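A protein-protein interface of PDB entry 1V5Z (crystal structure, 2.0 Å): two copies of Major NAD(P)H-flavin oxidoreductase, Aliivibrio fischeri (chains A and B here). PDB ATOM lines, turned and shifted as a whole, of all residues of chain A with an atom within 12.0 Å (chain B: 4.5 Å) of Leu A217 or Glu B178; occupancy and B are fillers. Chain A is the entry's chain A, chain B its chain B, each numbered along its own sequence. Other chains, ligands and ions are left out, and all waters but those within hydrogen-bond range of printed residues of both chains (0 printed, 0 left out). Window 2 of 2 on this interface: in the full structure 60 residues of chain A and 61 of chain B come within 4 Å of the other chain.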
ATOM      1  N   PHE A 210     -19.197  18.708  -2.105  1.00  0.00           N
ATOM      2  CA  PHE A 210     -20.433  19.383  -2.437  1.00  0.00           C
ATOM      3  C   PHE A 210     -20.233  20.899  -2.509  1.00  0.00           C
ATOM      4  O   PHE A 210     -20.683  21.543  -3.455  1.00  0.00           O
ATOM      5  CB  PHE A 210     -21.478  19.041  -1.384  1.00  0.00           C
ATOM      6  CG  PHE A 210     -22.831  19.658  -1.630  1.00  0.00           C
ATOM      7  CD1 PHE A 210     -23.916  18.858  -1.951  1.00  0.00           C
ATOM      8  CD2 PHE A 210     -23.032  21.024  -1.481  1.00  0.00           C
ATOM      9  CE1 PHE A 210     -25.176  19.410  -2.114  1.00  0.00           C
ATOM     10  CE2 PHE A 210     -24.281  21.579  -1.643  1.00  0.00           C
ATOM     11  CZ  PHE A 210     -25.355  20.771  -1.960  1.00  0.00           C
ATOM     12  N   GLU A 211     -19.553  21.467  -1.516  1.00  0.00           N
ATOM     13  CA  GLU A 211     -19.326  22.918  -1.473  1.00  0.00           C
ATOM     14  C   GLU A 211     -18.440  23.470  -2.595  1.00  0.00           C
ATOM     15  O   GLU A 211     -18.522  24.641  -2.914  1.00  0.00           O
ATOM     16  CB  GLU A 211     -18.798  23.358  -0.096  1.00  0.00           C
ATOM     17  CG  GLU A 211     -19.779  23.161   1.074  1.00  0.00           C
ATOM     18  CD  GLU A 211     -19.772  21.748   1.627  1.00  0.00           C
ATOM     19  OE1 GLU A 211     -18.869  20.960   1.254  1.00  0.00           O
ATOM     20  OE2 GLU A 211     -20.667  21.425   2.441  1.00  0.00           O
ATOM     21  N   ASP A 212     -17.615  22.616  -3.201  1.00  0.00           N
ATOM     22  CA  ASP A 212     -16.749  23.010  -4.318  1.00  0.00           C
ATOM     23  C   ASP A 212     -17.484  23.109  -5.659  1.00  0.00           C
ATOM     24  O   ASP A 212     -17.039  23.831  -6.544  1.00  0.00           O
ATOM     25  CB  ASP A 212     -15.582  22.033  -4.494  1.00  0.00           C
ATOM     26  CG  ASP A 212     -14.531  22.161  -3.411  1.00  0.00           C
ATOM     27  OD1 ASP A 212     -14.752  22.884  -2.414  1.00  0.00           O
ATOM     28  OD2 ASP A 212     -13.475  21.516  -3.554  1.00  0.00           O
ATOM     29  N   VAL A 213     -18.608  22.407  -5.817  1.00  0.00           N
ATOM     30  CA  VAL A 213     -19.318  22.431  -7.098  1.00  0.00           C
ATOM     31  C   VAL A 213     -20.708  23.001  -7.057  1.00  0.00           C
ATOM     32  O   VAL A 213     -21.242  23.342  -8.098  1.00  0.00           O
ATOM     33  CB  VAL A 213     -19.403  21.013  -7.757  1.00  0.00           C
ATOM     34  CG1 VAL A 213     -18.037  20.570  -8.229  1.00  0.00           C
ATOM     35  CG2 VAL A 213     -19.983  19.979  -6.757  1.00  0.00           C
ATOM     36  N   ILE A 214     -21.308  23.082  -5.874  1.00  0.00           N
ATOM     37  CA  ILE A 214     -22.666  23.608  -5.742  1.00  0.00           C
ATOM     38  C   ILE A 214     -22.717  24.855  -4.854  1.00  0.00           C
ATOM     39  O   ILE A 214     -22.147  24.876  -3.766  1.00  0.00           O
ATOM     40  CB  ILE A 214     -23.629  22.536  -5.154  1.00  0.00           C
ATOM     41  CG1 ILE A 214     -23.754  21.350  -6.120  1.00  0.00           C
ATOM     42  CG2 ILE A 214     -25.014  23.139  -4.895  1.00  0.00           C
ATOM     43  CD1 ILE A 214     -24.208  20.090  -5.465  1.00  0.00           C
ATOM     44  N   THR A 215     -23.405  25.886  -5.333  1.00  0.00           N
ATOM     45  CA  THR A 215     -23.547  27.122  -4.590  1.00  0.00           C
ATOM     46  C   THR A 215     -25.016  27.404  -4.516  1.00  0.00           C
ATOM     47  O   THR A 215     -25.693  27.386  -5.528  1.00  0.00           O
ATOM     48  CB  THR A 215     -22.919  28.314  -5.329  1.00  0.00           C
ATOM     49  OG1 THR A 215     -21.519  28.084  -5.530  1.00  0.00           O
ATOM     50  CG2 THR A 215     -23.122  29.595  -4.530  1.00  0.00           C
ATOM     51  N   ILE A 216     -25.509  27.695  -3.322  1.00  0.00           N
ATOM     52  CA  ILE A 216     -26.921  28.015  -3.145  1.00  0.00           C
ATOM     53  C   ILE A 216     -27.114  29.494  -2.767  1.00  0.00           C
ATOM     54  O   ILE A 216     -26.575  29.972  -1.762  1.00  0.00           O
ATOM     55  CB  ILE A 216     -27.567  27.074  -2.108  1.00  0.00           C
ATOM     56  CG1 ILE A 216     -27.420  25.619  -2.606  1.00  0.00           C
ATOM     57  CG2 ILE A 216     -29.021  27.447  -1.902  1.00  0.00           C
ATOM     58  CD1 ILE A 216     -27.892  24.533  -1.645  1.00  0.00           C
ATOM     59  N   LEU A 217     -27.873  30.205  -3.596  1.00  0.00           N
ATOM     60  CA  LEU A 217     -28.138  31.633  -3.396  1.00  0.00           C
ATOM     61  C   LEU A 217     -29.580  31.953  -2.984  1.00  0.00           C
ATOM     62  O   LEU A 217     -29.808  33.039  -2.410  1.00  0.00           O
ATOM     63  CB  LEU A 217     -27.774  32.418  -4.670  1.00  0.00           C
ATOM     64  CG  LEU A 217     -26.350  32.295  -5.224  1.00  0.00           C
ATOM     65  CD1 LEU A 217     -26.271  33.132  -6.486  1.00  0.00           C
ATOM     66  CD2 LEU A 217     -25.289  32.729  -4.224  1.00  0.00           C
ATOM     67  OXT LEU A 217     -30.481  31.132  -3.246  1.00  0.00           O
ATOM     68  N   LYS B  48     -19.849  24.047 -12.274  1.00  0.00           N
ATOM     69  CA  LYS B  48     -20.337  24.602 -11.025  1.00  0.00           C
ATOM     70  C   LYS B  48     -21.830  24.695 -11.254  1.00  0.00           C
ATOM     71  O   LYS B  48     -22.272  25.001 -12.356  1.00  0.00           O
ATOM     72  CB  LYS B  48     -19.742  25.997 -10.760  1.00  0.00           C
ATOM     73  CG  LYS B  48     -20.145  26.612  -9.437  1.00  0.00           C
ATOM     74  CD  LYS B  48     -19.691  28.073  -9.345  1.00  0.00           C
ATOM     75  CE  LYS B  48     -18.275  28.210  -8.831  1.00  0.00           C
ATOM     76  NZ  LYS B  48     -17.353  27.297  -9.537  1.00  0.00           N
ATOM     77  N   ILE B  50     -25.083  26.531  -9.819  1.00  0.00           N
ATOM     78  CA  ILE B  50     -25.585  27.603  -8.980  1.00  0.00           C
ATOM     79  C   ILE B  50     -27.098  27.500  -8.835  1.00  0.00           C
ATOM     80  O   ILE B  50     -27.832  27.641  -9.811  1.00  0.00           O
ATOM     81  CB  ILE B  50     -25.205  28.980  -9.578  1.00  0.00           C
ATOM     82  CG1 ILE B  50     -23.685  29.102  -9.645  1.00  0.00           C
ATOM     83  CG2 ILE B  50     -25.756  30.126  -8.726  1.00  0.00           C
ATOM     84  CD1 ILE B  50     -23.228  30.131 -10.645  1.00  0.00           C
ATOM     85  N   VAL B  51     -27.557  27.255  -7.609  1.00  0.00           N
ATOM     86  CA  VAL B  51     -28.986  27.122  -7.319  1.00  0.00           C
ATOM     87  C   VAL B  51     -29.569  28.456  -6.879  1.00  0.00           C
ATOM     88  O   VAL B  51     -29.171  29.013  -5.869  1.00  0.00           O
ATOM     89  CB  VAL B  51     -29.230  26.068  -6.200  1.00  0.00           C
ATOM     90  CG1 VAL B  51     -30.722  25.761  -6.061  1.00  0.00           C
ATOM     91  CG2 VAL B  51     -28.422  24.807  -6.476  1.00  0.00           C
ATOM     92  N   ILE B  52     -30.527  28.952  -7.641  1.00  0.00           N
ATOM     93  CA  ILE B  52     -31.180  30.208  -7.359  1.00  0.00           C
ATOM     94  C   ILE B  52     -32.385  29.843  -6.516  1.00  0.00           C
ATOM     95  O   ILE B  52     -33.393  29.414  -7.036  1.00  0.00           O
ATOM     96  CB  ILE B  52     -31.634  30.874  -8.677  1.00  0.00           C
ATOM     97  CG1 ILE B  52     -30.454  31.061  -9.658  1.00  0.00           C
ATOM     98  CG2 ILE B  52     -32.366  32.171  -8.410  1.00  0.00           C
ATOM     99  CD1 ILE B  52     -29.252  31.806  -9.133  1.00  0.00           C
ATOM    100  N   GLU B  53     -32.288  30.042  -5.211  1.00  0.00           N
ATOM    101  CA  GLU B  53     -33.368  29.672  -4.305  1.00  0.00           C
ATOM    102  C   GLU B  53     -34.094  30.808  -3.594  1.00  0.00           C
ATOM    103  O   GLU B  53     -35.325  30.845  -3.570  1.00  0.00           O
ATOM    104  CB  GLU B  53     -32.840  28.670  -3.284  1.00  0.00           C
ATOM    105  CG  GLU B  53     -33.819  28.331  -2.186  1.00  0.00           C
ATOM    106  CD  GLU B  53     -33.273  27.277  -1.264  1.00  0.00           C
ATOM    107  OE1 GLU B  53     -33.735  26.126  -1.346  1.00  0.00           O
ATOM    108  OE2 GLU B  53     -32.373  27.581  -0.468  1.00  0.00           O
ATOM    109  N   SER B  54     -33.346  31.716  -2.983  1.00  0.00           N
ATOM    110  CA  SER B  54     -33.953  32.836  -2.272  1.00  0.00           C
ATOM    111  C   SER B  54     -34.678  33.826  -3.183  1.00  0.00           C
ATOM    112  O   SER B  54     -34.456  33.865  -4.391  1.00  0.00           O
ATOM    113  CB  SER B  54     -32.884  33.578  -1.475  1.00  0.00           C
ATOM    114  OG  SER B  54     -32.005  34.257  -2.356  1.00  0.00           O
ATOM    115  N   ALA B  57     -32.237  36.105  -4.857  1.00  0.00           N
ATOM    116  CA  ALA B  57     -31.562  35.494  -5.989  1.00  0.00           C
ATOM    117  C   ALA B  57     -32.521  35.427  -7.175  1.00  0.00           C
ATOM    118  O   ALA B  57     -32.107  35.658  -8.299  1.00  0.00           O
ATOM    119  CB  ALA B  57     -31.048  34.101  -5.616  1.00  0.00           C
ATOM    120  N   ARG B  60     -32.541  38.748  -8.961  1.00  0.00           N
ATOM    121  CA  ARG B  60     -31.334  38.899  -9.769  1.00  0.00           C
ATOM    122  C   ARG B  60     -31.448  38.085 -11.052  1.00  0.00           C
ATOM    123  O   ARG B  60     -31.031  38.557 -12.109  1.00  0.00           O
ATOM    124  CB  ARG B  60     -30.091  38.445  -9.000  1.00  0.00           C
ATOM    125  CG  ARG B  60     -29.708  39.373  -7.847  1.00  0.00           C
ATOM    126  CD  ARG B  60     -28.710  38.739  -6.879  1.00  0.00           C
ATOM    127  NE  ARG B  60     -27.361  38.650  -7.427  1.00  0.00           N
ATOM    128  CZ  ARG B  60     -26.386  37.900  -6.918  1.00  0.00           C
ATOM    129  NH1 ARG B  60     -26.591  37.152  -5.834  1.00  0.00           N
ATOM    130  NH2 ARG B  60     -25.195  37.904  -7.494  1.00  0.00           N
ATOM    131  N   PHE B 175     -24.189  37.855 -11.655  1.00  0.00           N
ATOM    132  CA  PHE B 175     -23.637  36.844 -10.752  1.00  0.00           C
ATOM    133  C   PHE B 175     -22.140  36.871 -10.901  1.00  0.00           C
ATOM    134  O   PHE B 175     -21.474  35.832 -10.976  1.00  0.00           O
ATOM    135  CB  PHE B 175     -24.190  35.454 -11.081  1.00  0.00           C
ATOM    136  CG  PHE B 175     -25.668  35.338 -10.867  1.00  0.00           C
ATOM    137  CD1 PHE B 175     -26.541  35.412 -11.940  1.00  0.00           C
ATOM    138  CD2 PHE B 175     -26.188  35.201  -9.583  1.00  0.00           C
ATOM    139  CE1 PHE B 175     -27.900  35.360 -11.742  1.00  0.00           C
ATOM    140  CE2 PHE B 175     -27.544  35.148  -9.375  1.00  0.00           C
ATOM    141  CZ  PHE B 175     -28.404  35.229 -10.453  1.00  0.00           C
ATOM    142  N   ALA B 176     -21.629  38.097 -10.859  1.00  0.00           N
ATOM    143  CA  ALA B 176     -20.212  38.413 -11.019  1.00  0.00           C
ATOM    144  C   ALA B 176     -19.198  37.562 -10.283  1.00  0.00           C
ATOM    145  O   ALA B 176     -18.243  37.089 -10.893  1.00  0.00           O
ATOM    146  CB  ALA B 176     -19.978  39.881 -10.697  1.00  0.00           C
ATOM    147  N   ASP B 177     -19.382  37.392  -8.979  1.00  0.00           N
ATOM    148  CA  ASP B 177     -18.448  36.618  -8.160  1.00  0.00           C
ATOM    149  C   ASP B 177     -18.605  35.112  -8.327  1.00  0.00           C
ATOM    150  O   ASP B 177     -17.628  34.359  -8.237  1.00  0.00           O
ATOM    151  CB  ASP B 177     -18.661  36.904  -6.662  1.00  0.00           C
ATOM    152  CG  ASP B 177     -18.699  38.392  -6.325  1.00  0.00           C
ATOM    153  OD1 ASP B 177     -19.815  38.969  -6.313  1.00  0.00           O
ATOM    154  OD2 ASP B 177     -17.622  38.964  -6.040  1.00  0.00           O
ATOM    155  N   GLU B 178     -19.855  34.684  -8.496  1.00  0.00           N
ATOM    156  CA  GLU B 178     -20.214  33.275  -8.630  1.00  0.00           C
ATOM    157  C   GLU B 178     -19.780  32.625  -9.947  1.00  0.00           C
ATOM    158  O   GLU B 178     -19.328  31.477  -9.978  1.00  0.00           O
ATOM    159  CB  GLU B 178     -21.719  33.119  -8.430  1.00  0.00           C
ATOM    160  CG  GLU B 178     -22.229  33.655  -7.090  1.00  0.00           C
ATOM    161  CD  GLU B 178     -22.741  35.105  -7.140  1.00  0.00           C
ATOM    162  OE1 GLU B 178     -22.316  35.903  -8.002  1.00  0.00           O
ATOM    163  OE2 GLU B 178     -23.587  35.454  -6.297  1.00  0.00           O
ATOM    164  N   LEU B 179     -19.889  33.376 -11.028  1.00  0.00           N
ATOM    165  CA  LEU B 179     -19.513  32.881 -12.337  1.00  0.00           C
ATOM    166  C   LEU B 179     -18.082  33.257 -12.728  1.00  0.00           C
ATOM    167  O   LEU B 179     -17.715  33.185 -13.906  1.00  0.00           O
ATOM    168  CB  LEU B 179     -20.504  33.402 -13.379  1.00  0.00           C
ATOM    169  CG  LEU B 179     -21.923  32.865 -13.206  1.00  0.00           C
ATOM    170  CD1 LEU B 179     -22.873  33.494 -14.207  1.00  0.00           C
ATOM    171  CD2 LEU B 179     -21.893  31.370 -13.397  1.00  0.00           C
ATOM    172  N   LYS B 180     -17.268  33.621 -11.736  1.00  0.00           N
ATOM    173  CA  LYS B 180     -15.885  34.014 -11.991  1.00  0.00           C
ATOM    174  C   LYS B 180     -15.061  32.826 -12.446  1.00  0.00           C
ATOM    175  O   LYS B 180     -14.835  31.892 -11.677  1.00  0.00           O
ATOM    176  CB  LYS B 180     -15.259  34.630 -10.740  1.00  0.00           C
ATOM    177  CG  LYS B 180     -13.859  35.198 -10.945  1.00  0.00           C
ATOM    178  CD  LYS B 180     -13.400  35.960  -9.708  1.00  0.00           C
ATOM    179  CE  LYS B 180     -14.387  37.082  -9.347  1.00  0.00           C
ATOM    180  NZ  LYS B 180     -14.580  38.081 -10.459  1.00  0.00           N
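O of Thr A215 lies within hydrogen-bond range of N of Val B51 (2.8 Å).
The backbone NH of Leu A217 is in hydrogen-bond range of the backbone carbonyl oxygen of Val B51 (2.9 Å).
The chain-end carboxylate (OXT) of Leu A217 sits at hydrogen-bond distance from the backbone NH (N) of Glu B53, at 2.9 Å.
The chain-end carboxylate (O) of Leu A217 sits at hydrogen-bond distance from the side-chain hydroxyl (OG) of Ser B54 (2.5 Å).
Of the printed residues of chain B, Val A213 touches Lys B48.
Ile A214 touches none of the printed residues of chain B.
Of the printed residues of chain B, Thr A215 touches Ile B50 and Val B51.
Printed residues of chain B within 4 Å of Ile A216: Val B51 (3.7 Å) and Glu B53 (3.6 Å).
Of the printed residues of chain B, Leu A217 touches Ile B50 (3.8 Å), Val B51 (2.9 Å), Ile B52 (3.997 Å), Glu B53 (2.9 Å), Ser B54 (2.5 Å), Ala B57 (3.6 Å), Phe B175 (3.7 Å) and Glu B178 (3.6 Å).
Lys B48 touches just one residue of chain A: Val A213 (3.3 Å).
Val B51 touches three residues of chain A.
Printed residues of chain A within 4 Å of Ile B52: Leu A217 (3.997 Å).
Of the printed residues of chain A, Glu B53 touches Ile A216 and Leu A217.
Ser B54 touches one residue of chain A.
Ala B57 touches one residue of chain A.
No residue of chain A comes within 4 Å of Asp B177.
Glu B178 touches one residue of chain A.
No residue of chain A comes within 4 Å of Leu B179.
The nearest residue of chain A that does not touch Glu B178 is Thr A215 (4.9 Å).
The side-chain hydroxyl (OG) of Ser B54 is in hydrogen-bond range of the backbone NH (N) of Ala B57 (3.1 Å).
The guanidinium group (NH2) of Arg B60 lies within salt-bridge range of the side-chain carboxylate (OE2) of Glu B178 (3.2 Å).
Among the printed residues, merely in contact across the chains: Val A213 with Lys B48, Thr A215 with Ile B50, Ile A216 with Val B51, Ile A216 with Glu B53, Leu A217 with Ile B50, Leu A217 with Ile B52, Leu A217 with Ala B57, Leu A217 with Phe B175 and Leu A217 with Glu B178.
No position is printed for both chains.
Of the 13 pairs that touch across the chains among the printed residues, none has its exchanged pair printed and touching as well.
Of the 14 printed residues of chain B, 9 touch a printed residue of chain A.
Of the 8 printed residues of chain A, 4 touch a printed residue of chain B.
Hydrophobic or aromatic side chains of chain A within 4 Å of the printed part of chain B: Ile A216 and Leu A217.
Among the printed residues, 13 pairs touch across the chains.
Among the printed residues, no Asp or Glu carboxylate lies within 4 Å of a Lys or Arg side-chain nitrogen of the other chain.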
